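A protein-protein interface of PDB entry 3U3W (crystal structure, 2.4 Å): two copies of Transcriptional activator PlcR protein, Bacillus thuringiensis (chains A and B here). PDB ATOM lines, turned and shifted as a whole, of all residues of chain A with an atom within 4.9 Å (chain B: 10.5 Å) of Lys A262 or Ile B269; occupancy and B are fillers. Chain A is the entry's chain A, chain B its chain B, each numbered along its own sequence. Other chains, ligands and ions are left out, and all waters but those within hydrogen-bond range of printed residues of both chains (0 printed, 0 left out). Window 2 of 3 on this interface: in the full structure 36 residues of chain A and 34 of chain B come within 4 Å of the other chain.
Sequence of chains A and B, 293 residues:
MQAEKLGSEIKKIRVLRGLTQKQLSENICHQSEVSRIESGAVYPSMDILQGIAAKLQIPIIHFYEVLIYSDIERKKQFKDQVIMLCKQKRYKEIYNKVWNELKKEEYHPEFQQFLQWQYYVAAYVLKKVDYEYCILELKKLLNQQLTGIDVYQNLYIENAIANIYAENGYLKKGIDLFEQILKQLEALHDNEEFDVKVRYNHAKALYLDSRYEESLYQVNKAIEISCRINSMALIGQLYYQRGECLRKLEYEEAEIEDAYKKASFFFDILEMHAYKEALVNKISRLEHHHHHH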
ATOM      1  N   CYS A 227      13.998  28.326   1.652  1.00  0.00           N
ATOM      2  CA  CYS A 227      12.737  27.787   1.131  1.00  0.00           C
ATOM      3  C   CYS A 227      12.707  27.635  -0.398  1.00  0.00           C
ATOM      4  O   CYS A 227      12.217  26.643  -0.919  1.00  0.00           O
ATOM      5  CB  CYS A 227      11.549  28.604   1.626  1.00  0.00           C
ATOM      6  SG  CYS A 227      11.382  28.508   3.416  1.00  0.00           S
ATOM      7  N   TYR A 239      15.243  30.227  11.986  1.00  0.00           N
ATOM      8  CA  TYR A 239      14.051  30.509  12.771  1.00  0.00           C
ATOM      9  C   TYR A 239      14.360  30.861  14.209  1.00  0.00           C
ATOM     10  O   TYR A 239      13.695  31.708  14.783  1.00  0.00           O
ATOM     11  CB  TYR A 239      13.066  29.343  12.739  1.00  0.00           C
ATOM     12  CG  TYR A 239      12.301  29.306  11.456  1.00  0.00           C
ATOM     13  CD1 TYR A 239      11.500  30.373  11.074  1.00  0.00           C
ATOM     14  CD2 TYR A 239      12.409  28.224  10.603  1.00  0.00           C
ATOM     15  CE1 TYR A 239      10.810  30.356   9.879  1.00  0.00           C
ATOM     16  CE2 TYR A 239      11.730  28.195   9.412  1.00  0.00           C
ATOM     17  CZ  TYR A 239      10.929  29.262   9.055  1.00  0.00           C
ATOM     18  OH  TYR A 239      10.255  29.210   7.859  1.00  0.00           O
ATOM     19  N   ASP A 258       6.046  31.794  17.472  1.00  0.00           N
ATOM     20  CA  ASP A 258       6.013  31.136  16.168  1.00  0.00           C
ATOM     21  C   ASP A 258       7.409  30.756  15.694  1.00  0.00           C
ATOM     22  O   ASP A 258       7.646  29.610  15.316  1.00  0.00           O
ATOM     23  CB  ASP A 258       5.355  32.043  15.116  1.00  0.00           C
ATOM     24  CG  ASP A 258       5.162  31.342  13.776  1.00  0.00           C
ATOM     25  OD1 ASP A 258       4.367  30.381  13.711  1.00  0.00           O
ATOM     26  OD2 ASP A 258       5.795  31.759  12.782  1.00  0.00           O
ATOM     27  N   ALA A 259       8.325  31.724  15.706  1.00  0.00           N
ATOM     28  CA  ALA A 259       9.661  31.485  15.194  1.00  0.00           C
ATOM     29  C   ALA A 259      10.328  30.360  15.960  1.00  0.00           C
ATOM     30  O   ALA A 259      10.898  29.452  15.354  1.00  0.00           O
ATOM     31  CB  ALA A 259      10.502  32.745  15.233  1.00  0.00           C
ATOM     32  N   TYR A 260      10.238  30.403  17.288  1.00  0.00           N
ATOM     33  CA  TYR A 260      10.877  29.382  18.126  1.00  0.00           C
ATOM     34  C   TYR A 260      10.263  27.986  17.936  1.00  0.00           C
ATOM     35  O   TYR A 260      10.970  26.978  17.999  1.00  0.00           O
ATOM     36  CB  TYR A 260      10.848  29.785  19.603  1.00  0.00           C
ATOM     37  CG  TYR A 260      11.796  30.904  19.989  1.00  0.00           C
ATOM     38  CD1 TYR A 260      13.165  30.808  19.734  1.00  0.00           C
ATOM     39  CD2 TYR A 260      11.331  32.048  20.633  1.00  0.00           C
ATOM     40  CE1 TYR A 260      14.042  31.828  20.093  1.00  0.00           C
ATOM     41  CE2 TYR A 260      12.201  33.073  21.003  1.00  0.00           C
ATOM     42  CZ  TYR A 260      13.554  32.954  20.732  1.00  0.00           C
ATOM     43  OH  TYR A 260      14.415  33.964  21.091  1.00  0.00           O
ATOM     44  N   LYS A 261       8.951  27.933  17.699  1.00  0.00           N
ATOM     45  CA  LYS A 261       8.270  26.668  17.426  1.00  0.00           C
ATOM     46  C   LYS A 261       8.774  26.053  16.127  1.00  0.00           C
ATOM     47  O   LYS A 261       9.060  24.855  16.057  1.00  0.00           O
ATOM     48  CB  LYS A 261       6.754  26.857  17.368  1.00  0.00           C
ATOM     49  CG  LYS A 261       6.101  27.000  18.738  1.00  0.00           C
ATOM     50  CD  LYS A 261       4.665  27.513  18.623  1.00  0.00           C
ATOM     51  CE  LYS A 261       3.716  26.455  18.064  1.00  0.00           C
ATOM     52  NZ  LYS A 261       4.038  26.031  16.665  1.00  0.00           N
ATOM     53  N   LYS A 262       8.895  26.881  15.101  1.00  0.00           N
ATOM     54  CA  LYS A 262       9.443  26.416  13.841  1.00  0.00           C
ATOM     55  C   LYS A 262      10.864  25.867  14.020  1.00  0.00           C
ATOM     56  O   LYS A 262      11.221  24.862  13.405  1.00  0.00           O
ATOM     57  CB  LYS A 262       9.391  27.522  12.786  1.00  0.00           C
ATOM     58  CG  LYS A 262       7.979  27.831  12.283  1.00  0.00           C
ATOM     59  CD  LYS A 262       8.022  28.998  11.295  1.00  0.00           C
ATOM     60  CE  LYS A 262       6.763  29.099  10.442  1.00  0.00           C
ATOM     61  NZ  LYS A 262       5.527  29.326  11.235  1.00  0.00           N
ATOM     62  N   ALA A 263      11.666  26.507  14.871  1.00  0.00           N
ATOM     63  CA  ALA A 263      13.023  26.029  15.127  1.00  0.00           C
ATOM     64  C   ALA A 263      13.002  24.688  15.829  1.00  0.00           C
ATOM     65  O   ALA A 263      13.720  23.775  15.445  1.00  0.00           O
ATOM     66  CB  ALA A 263      13.822  27.042  15.948  1.00  0.00           C
ATOM     67  N   SER A 264      12.175  24.591  16.866  1.00  0.00           N
ATOM     68  CA  SER A 264      11.990  23.354  17.632  1.00  0.00           C
ATOM     69  C   SER A 264      11.517  22.193  16.743  1.00  0.00           C
ATOM     70  O   SER A 264      11.970  21.057  16.893  1.00  0.00           O
ATOM     71  CB  SER A 264      11.001  23.584  18.785  1.00  0.00           C
ATOM     72  OG  SER A 264      10.866  22.431  19.605  1.00  0.00           O
ATOM     73  N   PHE A 265      10.617  22.487  15.810  1.00  0.00           N
ATOM     74  CA  PHE A 265      10.249  21.511  14.804  1.00  0.00           C
ATOM     75  C   PHE A 265      11.472  20.948  14.072  1.00  0.00           C
ATOM     76  O   PHE A 265      11.662  19.734  14.037  1.00  0.00           O
ATOM     77  CB  PHE A 265       9.254  22.090  13.796  1.00  0.00           C
ATOM     78  CG  PHE A 265       8.698  21.057  12.836  1.00  0.00           C
ATOM     79  CD1 PHE A 265       9.407  20.695  11.693  1.00  0.00           C
ATOM     80  CD2 PHE A 265       7.479  20.434  13.086  1.00  0.00           C
ATOM     81  CE1 PHE A 265       8.913  19.738  10.816  1.00  0.00           C
ATOM     82  CE2 PHE A 265       6.975  19.487  12.205  1.00  0.00           C
ATOM     83  CZ  PHE A 265       7.696  19.139  11.067  1.00  0.00           C
ATOM     84  N   PHE A 266      12.292  21.811  13.477  1.00  0.00           N
ATOM     85  CA  PHE A 266      13.439  21.333  12.703  1.00  0.00           C
ATOM     86  C   PHE A 266      14.486  20.643  13.544  1.00  0.00           C
ATOM     87  O   PHE A 266      15.036  19.624  13.126  1.00  0.00           O
ATOM     88  CB  PHE A 266      14.074  22.447  11.872  1.00  0.00           C
ATOM     89  CG  PHE A 266      13.254  22.829  10.692  1.00  0.00           C
ATOM     90  CD1 PHE A 266      13.176  21.988   9.584  1.00  0.00           C
ATOM     91  CD2 PHE A 266      12.526  24.003  10.690  1.00  0.00           C
ATOM     92  CE1 PHE A 266      12.384  22.324   8.488  1.00  0.00           C
ATOM     93  CE2 PHE A 266      11.740  24.350   9.595  1.00  0.00           C
ATOM     94  CZ  PHE A 266      11.665  23.501   8.497  1.00  0.00           C
ATOM     95  N   SER B 231      17.282  18.086   2.310  1.00  0.00           N
ATOM     96  CA  SER B 231      16.290  18.495   1.319  1.00  0.00           C
ATOM     97  C   SER B 231      14.855  18.529   1.876  1.00  0.00           C
ATOM     98  O   SER B 231      14.440  17.637   2.600  1.00  0.00           O
ATOM     99  CB  SER B 231      16.355  17.564   0.109  1.00  0.00           C
ATOM    100  OG  SER B 231      15.617  18.100  -0.962  1.00  0.00           O
ATOM    101  N   MET B 232      14.117  19.579   1.528  1.00  0.00           N
ATOM    102  CA  MET B 232      12.716  19.736   1.904  1.00  0.00           C
ATOM    103  C   MET B 232      11.841  19.503   0.690  1.00  0.00           C
ATOM    104  O   MET B 232      10.623  19.600   0.790  1.00  0.00           O
ATOM    105  CB  MET B 232      12.414  21.180   2.320  1.00  0.00           C
ATOM    106  CG  MET B 232      13.152  21.723   3.480  1.00  0.00           C
ATOM    107  SD  MET B 232      12.275  23.148   4.130  1.00  0.00           S
ATOM    108  CE  MET B 232      13.123  24.480   3.281  1.00  0.00           C
ATOM    109  N   ALA B 233      12.454  19.269  -0.466  1.00  0.00           N
ATOM    110  CA  ALA B 233      11.713  19.284  -1.732  1.00  0.00           C
ATOM    111  C   ALA B 233      10.452  18.400  -1.682  1.00  0.00           C
ATOM    112  O   ALA B 233       9.361  18.810  -2.074  1.00  0.00           O
ATOM    113  CB  ALA B 233      12.620  18.859  -2.886  1.00  0.00           C
ATOM    114  N   ILE B 235       9.670  16.338   1.249  1.00  0.00           N
ATOM    115  CA  ILE B 235       9.570  15.768   2.598  1.00  0.00           C
ATOM    116  C   ILE B 235       8.176  15.870   3.228  1.00  0.00           C
ATOM    117  O   ILE B 235       7.782  15.000   4.003  1.00  0.00           O
ATOM    118  CB  ILE B 235      10.670  16.315   3.581  1.00  0.00           C
ATOM    119  CG1 ILE B 235      10.736  15.429   4.824  1.00  0.00           C
ATOM    120  CG2 ILE B 235      10.370  17.747   4.004  1.00  0.00           C
ATOM    121  CD1 ILE B 235      12.116  15.066   5.250  1.00  0.00           C
ATOM    122  N   GLY B 236       7.445  16.940   2.922  1.00  0.00           N
ATOM    123  CA  GLY B 236       6.054  17.049   3.333  1.00  0.00           C
ATOM    124  C   GLY B 236       5.201  15.951   2.694  1.00  0.00           C
ATOM    125  O   GLY B 236       4.466  15.247   3.377  1.00  0.00           O
ATOM    126  N   GLN B 237       5.317  15.803   1.379  1.00  0.00           N
ATOM    127  CA  GLN B 237       4.618  14.754   0.647  1.00  0.00           C
ATOM    128  C   GLN B 237       4.949  13.381   1.238  1.00  0.00           C
ATOM    129  O   GLN B 237       4.062  12.557   1.437  1.00  0.00           O
ATOM    130  CB  GLN B 237       4.982  14.783  -0.843  1.00  0.00           C
ATOM    131  CG  GLN B 237       4.636  16.062  -1.574  1.00  0.00           C
ATOM    132  CD  GLN B 237       5.779  17.103  -1.515  1.00  0.00           C
ATOM    133  OE1 GLN B 237       6.313  17.390  -0.447  1.00  0.00           O
ATOM    134  NE2 GLN B 237       6.151  17.657  -2.672  1.00  0.00           N
ATOM    135  N   LYS B 261       0.705  15.625  10.909  1.00  0.00           N
ATOM    136  CA  LYS B 261       1.074  16.935  11.467  1.00  0.00           C
ATOM    137  C   LYS B 261       2.385  17.442  10.867  1.00  0.00           C
ATOM    138  O   LYS B 261       2.503  18.612  10.505  1.00  0.00           O
ATOM    139  CB  LYS B 261       1.179  16.895  12.994  1.00  0.00           C
ATOM    140  CG  LYS B 261      -0.164  16.702  13.695  1.00  0.00           C
ATOM    141  CD  LYS B 261       0.011  16.617  15.206  1.00  0.00           C
ATOM    142  CE  LYS B 261       0.453  17.959  15.797  1.00  0.00           C
ATOM    143  NZ  LYS B 261      -0.536  19.063  15.563  1.00  0.00           N
ATOM    144  N   LYS B 262       3.354  16.546  10.754  1.00  0.00           N
ATOM    145  CA  LYS B 262       4.621  16.856  10.117  1.00  0.00           C
ATOM    146  C   LYS B 262       4.444  17.323   8.663  1.00  0.00           C
ATOM    147  O   LYS B 262       5.129  18.253   8.220  1.00  0.00           O
ATOM    148  CB  LYS B 262       5.554  15.652  10.194  1.00  0.00           C
ATOM    149  CG  LYS B 262       6.135  15.380  11.575  1.00  0.00           C
ATOM    150  CD  LYS B 262       7.039  14.138  11.536  1.00  0.00           C
ATOM    151  CE  LYS B 262       8.130  14.147  12.605  1.00  0.00           C
ATOM    152  NZ  LYS B 262       7.619  14.101  13.998  1.00  0.00           N
ATOM    153  N   ALA B 263       3.529  16.694   7.927  1.00  0.00           N
ATOM    154  CA  ALA B 263       3.260  17.100   6.544  1.00  0.00           C
ATOM    155  C   ALA B 263       2.641  18.477   6.513  1.00  0.00           C
ATOM    156  O   ALA B 263       3.005  19.317   5.702  1.00  0.00           O
ATOM    157  CB  ALA B 263       2.336  16.101   5.848  1.00  0.00           C
ATOM    158  N   SER B 264       1.688  18.691   7.405  1.00  0.00           N
ATOM    159  CA  SER B 264       1.013  19.968   7.516  1.00  0.00           C
ATOM    160  C   SER B 264       2.028  21.081   7.812  1.00  0.00           C
ATOM    161  O   SER B 264       1.894  22.204   7.319  1.00  0.00           O
ATOM    162  CB  SER B 264      -0.072  19.895   8.597  1.00  0.00           C
ATOM    163  OG  SER B 264      -0.770  21.126   8.718  1.00  0.00           O
ATOM    164  N   PHE B 265       3.054  20.760   8.597  1.00  0.00           N
ATOM    165  CA  PHE B 265       4.098  21.732   8.898  1.00  0.00           C
ATOM    166  C   PHE B 265       4.820  22.212   7.628  1.00  0.00           C
ATOM    167  O   PHE B 265       4.946  23.409   7.399  1.00  0.00           O
ATOM    168  CB  PHE B 265       5.108  21.161   9.897  1.00  0.00           C
ATOM    169  CG  PHE B 265       6.210  22.138  10.270  1.00  0.00           C
ATOM    170  CD1 PHE B 265       7.326  22.299   9.452  1.00  0.00           C
ATOM    171  CD2 PHE B 265       6.118  22.909  11.424  1.00  0.00           C
ATOM    172  CE1 PHE B 265       8.333  23.208   9.783  1.00  0.00           C
ATOM    173  CE2 PHE B 265       7.125  23.809  11.763  1.00  0.00           C
ATOM    174  CZ  PHE B 265       8.234  23.955  10.947  1.00  0.00           C
ATOM    175  N   PHE B 266       5.290  21.276   6.808  1.00  0.00           N
ATOM    176  CA  PHE B 266       6.047  21.632   5.615  1.00  0.00           C
ATOM    177  C   PHE B 266       5.184  22.271   4.544  1.00  0.00           C
ATOM    178  O   PHE B 266       5.659  23.118   3.786  1.00  0.00           O
ATOM    179  CB  PHE B 266       6.769  20.420   5.042  1.00  0.00           C
ATOM    180  CG  PHE B 266       7.955  20.001   5.842  1.00  0.00           C
ATOM    181  CD1 PHE B 266       9.155  20.702   5.749  1.00  0.00           C
ATOM    182  CD2 PHE B 266       7.887  18.900   6.678  1.00  0.00           C
ATOM    183  CE1 PHE B 266      10.261  20.324   6.494  1.00  0.00           C
ATOM    184  CE2 PHE B 266       8.989  18.518   7.420  1.00  0.00           C
ATOM    185  CZ  PHE B 266      10.180  19.239   7.332  1.00  0.00           C
ATOM    186  N   PHE B 267       3.921  21.857   4.465  1.00  0.00           N
ATOM    187  CA  PHE B 267       3.013  22.478   3.508  1.00  0.00           C
ATOM    188  C   PHE B 267       2.814  23.951   3.875  1.00  0.00           C
ATOM    189  O   PHE B 267       2.777  24.813   3.003  1.00  0.00           O
ATOM    190  CB  PHE B 267       1.667  21.744   3.425  1.00  0.00           C
ATOM    191  CG  PHE B 267       1.762  20.343   2.858  1.00  0.00           C
ATOM    192  CD1 PHE B 267       2.900  19.920   2.185  1.00  0.00           C
ATOM    193  CD2 PHE B 267       0.706  19.451   3.003  1.00  0.00           C
ATOM    194  CE1 PHE B 267       2.989  18.625   1.673  1.00  0.00           C
ATOM    195  CE2 PHE B 267       0.784  18.158   2.496  1.00  0.00           C
ATOM    196  CZ  PHE B 267       1.927  17.744   1.839  1.00  0.00           C
ATOM    197  N   ASP B 268       2.682  24.232   5.170  1.00  0.00           N
ATOM    198  CA  ASP B 268       2.520  25.606   5.628  1.00  0.00           C
ATOM    199  C   ASP B 268       3.721  26.441   5.211  1.00  0.00           C
ATOM    200  O   ASP B 268       3.596  27.343   4.384  1.00  0.00           O
ATOM    201  CB  ASP B 268       2.314  25.684   7.149  1.00  0.00           C
ATOM    202  CG  ASP B 268       2.172  27.125   7.651  1.00  0.00           C
ATOM    203  OD1 ASP B 268       1.137  27.754   7.342  1.00  0.00           O
ATOM    204  OD2 ASP B 268       3.090  27.631   8.349  1.00  0.00           O
ATOM    205  N   ILE B 269       4.890  26.132   5.767  1.00  0.00           N
ATOM    206  CA  ILE B 269       6.065  26.987   5.538  1.00  0.00           C
ATOM    207  C   ILE B 269       6.543  27.035   4.097  1.00  0.00           C
ATOM    208  O   ILE B 269       7.115  28.040   3.688  1.00  0.00           O
ATOM    209  CB  ILE B 269       7.277  26.697   6.463  1.00  0.00           C
ATOM    210  CG1 ILE B 269       7.947  25.380   6.092  1.00  0.00           C
ATOM    211  CG2 ILE B 269       6.887  26.764   7.933  1.00  0.00           C
ATOM    212  CD1 ILE B 269       9.436  25.525   5.931  1.00  0.00           C
ATOM    213  N   LEU B 270       6.318  25.972   3.327  1.00  0.00           N
ATOM    214  CA  LEU B 270       6.685  26.001   1.913  1.00  0.00           C
ATOM    215  C   LEU B 270       5.535  26.547   1.054  1.00  0.00           C
ATOM    216  O   LEU B 270       5.642  26.656  -0.166  1.00  0.00           O
ATOM    217  CB  LEU B 270       7.148  24.627   1.428  1.00  0.00           C
ATOM    218  CG  LEU B 270       8.377  24.097   2.161  1.00  0.00           C
ATOM    219  CD1 LEU B 270       8.782  22.725   1.612  1.00  0.00           C
ATOM    220  CD2 LEU B 270       9.521  25.104   2.039  1.00  0.00           C
ATOM    221  N   GLU B 271       4.434  26.897   1.707  1.00  0.00           N
ATOM    222  CA  GLU B 271       3.320  27.525   1.011  1.00  0.00           C
ATOM    223  C   GLU B 271       2.780  26.646  -0.113  1.00  0.00           C
ATOM    224  O   GLU B 271       2.481  27.133  -1.208  1.00  0.00           O
ATOM    225  CB  GLU B 271       3.753  28.880   0.450  1.00  0.00           C
ATOM    226  CG  GLU B 271       4.228  29.859   1.511  1.00  0.00           C
ATOM    227  CD  GLU B 271       4.660  31.182   0.917  1.00  0.00           C
ATOM    228  OE1 GLU B 271       5.866  31.330   0.617  1.00  0.00           O
ATOM    229  OE2 GLU B 271       3.793  32.069   0.743  1.00  0.00           O
ATOM    230  N   MET B 272       2.674  25.349   0.157  1.00  0.00           N
ATOM    231  CA  MET B 272       2.106  24.411  -0.806  1.00  0.00           C
ATOM    232  C   MET B 272       0.581  24.361  -0.611  1.00  0.00           C
ATOM    233  O   MET B 272       0.044  23.444   0.023  1.00  0.00           O
ATOM    234  CB  MET B 272       2.760  23.032  -0.643  1.00  0.00           C
ATOM    235  CG  MET B 272       4.258  23.024  -0.958  1.00  0.00           C
ATOM    236  SD  MET B 272       5.252  21.745  -0.139  1.00  0.00           S
ATOM    237  CE  MET B 272       4.762  20.289  -1.056  1.00  0.00           C
ATOM    238  N   HIS B 273      -0.109  25.367  -1.150  1.00  0.00           N
ATOM    239  CA  HIS B 273      -1.540  25.561  -0.888  1.00  0.00           C
ATOM    240  C   HIS B 273      -2.394  24.429  -1.452  1.00  0.00           C
ATOM    241  O   HIS B 273      -3.263  23.894  -0.755  1.00  0.00           O
ATOM    242  CB  HIS B 273      -2.014  26.916  -1.420  1.00  0.00           C
ATOM    243  CG  HIS B 273      -1.268  28.080  -0.848  1.00  0.00           C
ATOM    244  ND1 HIS B 273      -1.301  28.397   0.494  1.00  0.00           N
ATOM    245  CD2 HIS B 273      -0.463  28.999  -1.435  1.00  0.00           C
ATOM    246  CE1 HIS B 273      -0.547  29.462   0.709  1.00  0.00           C
ATOM    247  NE2 HIS B 273      -0.027  29.847  -0.444  1.00  0.00           N
ATOM    248  N   TYR B 275      -1.624  21.249  -1.919  1.00  0.00           N
ATOM    249  CA  TYR B 275      -1.468  20.064  -1.067  1.00  0.00           C
ATOM    250  C   TYR B 275      -2.249  20.127   0.242  1.00  0.00           C
ATOM    251  O   TYR B 275      -2.531  19.094   0.845  1.00  0.00           O
ATOM    252  CB  TYR B 275       0.015  19.827  -0.733  1.00  0.00           C
ATOM    253  CG  TYR B 275       0.920  19.558  -1.912  1.00  0.00           C
ATOM    254  CD1 TYR B 275       1.085  20.485  -2.918  1.00  0.00           C
ATOM    255  CD2 TYR B 275       1.632  18.381  -1.999  1.00  0.00           C
ATOM    256  CE1 TYR B 275       1.922  20.237  -3.988  1.00  0.00           C
ATOM    257  CE2 TYR B 275       2.472  18.127  -3.063  1.00  0.00           C
ATOM    258  CZ  TYR B 275       2.612  19.055  -4.053  1.00  0.00           C
ATOM    259  OH  TYR B 275       3.465  18.797  -5.104  1.00  0.00           O
ATOM    260  N   LYS B 276      -2.569  21.327   0.709  1.00  0.00           N
ATOM    261  CA  LYS B 276      -3.226  21.468   2.009  1.00  0.00           C
ATOM    262  C   LYS B 276      -4.632  20.884   1.995  1.00  0.00           C
ATOM    263  O   LYS B 276      -5.169  20.473   3.029  1.00  0.00           O
ATOM    264  CB  LYS B 276      -3.274  22.933   2.426  1.00  0.00           C
ATOM    265  CG  LYS B 276      -1.986  23.438   3.042  1.00  0.00           C
ATOM    266  CD  LYS B 276      -1.744  24.884   2.659  1.00  0.00           C
ATOM    267  CE  LYS B 276      -1.225  25.700   3.826  1.00  0.00           C
ATOM    268  NZ  LYS B 276      -0.988  27.121   3.422  1.00  0.00           N
ATOM    269  N   LEU B 279      -5.269  17.376   3.295  1.00  0.00           N
ATOM    270  CA  LEU B 279      -5.085  17.152   4.723  1.00  0.00           C
ATOM    271  C   LEU B 279      -6.360  17.290   5.551  1.00  0.00           C
ATOM    272  O   LEU B 279      -6.307  17.248   6.781  1.00  0.00           O
ATOM    273  CB  LEU B 279      -3.990  18.057   5.268  1.00  0.00           C
ATOM    274  CG  LEU B 279      -2.584  17.467   5.203  1.00  0.00           C
ATOM    275  CD1 LEU B 279      -1.573  18.547   5.505  1.00  0.00           C
ATOM    276  CD2 LEU B 279      -2.442  16.304   6.182  1.00  0.00           C
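Among the printed residues, merely in contact across the chains: Cys A227 with Met B232 (3.96 Å), Lys A262 with Phe B265 (3.97 Å), Lys A262 with Ile B269 (3.4 Å), Phe A265 with Lys B262 (3.9 Å), Phe A265 with Phe B265 (3.3 Å), Phe A265 with Phe B266 (3.6 Å), Phe A266 with Phe B265 (3.6 Å), Phe A266 with Phe B266 (3.5 Å) and Phe A266 with Ile B269 (3.96 Å).
Of the printed residues of chain B, Cys A227 touches Met B232. No residue of chain B comes within 4 Å of Lys A261. Of chain B, only Phe B265 and Ile B269 come within 4 Å of Lys A262. No residue of chain B comes within 4 Å of Ala A263. Printed residues of chain B within 4 Å of Phe A265: Lys B262, Phe B265 and Phe B266. Of the printed residues of chain A, Phe B265 touches Lys A262 (3.97 Å), Phe A265 (3.3 Å) and Phe A266 (3.6 Å). Asp B268 touches none of the printed residues of chain A. Of chain A, only Lys A262 and Phe A266 come within 4 Å of Ile B269. Met B272 touches none of the printed residues of chain A. The nearest residue of chain A that does not touch Ile B269 is Tyr A239 (4.1 Å).
Of the 11 printed residues of chain A, 4 touch a printed residue of chain B. Hydrophobic or aromatic side chains of chain A that line the printed part of chain B: Phe A265 and Phe A266. Of the 22 printed residues of chain B, 5 touch a printed residue of chain A. Hydrophobic or aromatic side chains of chain B within 4 Å of the printed part of chain A: Met B232, Phe B265, Phe B266 and Ile B269. Among the printed residues, no Asp or Glu carboxylate lies within 4 Å of a Lys or Arg side-chain nitrogen of the other chain.
OD2 of Asp A258 is in salt-bridge range of NZ of Lys A262 (2.9 Å).
Lys A262 touches Phe B265, and with the chains exchanged Phe A265 touches Lys B262. Phe A265 touches its own counterpart, Phe B265. Phe A265 touches Phe B266, and with the chains exchanged Phe A266 touches Phe B265. Phe A266 touches its own counterpart, Phe B266. Positions printed for both chains: 261, 262, 263, 264, 265 and 266.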
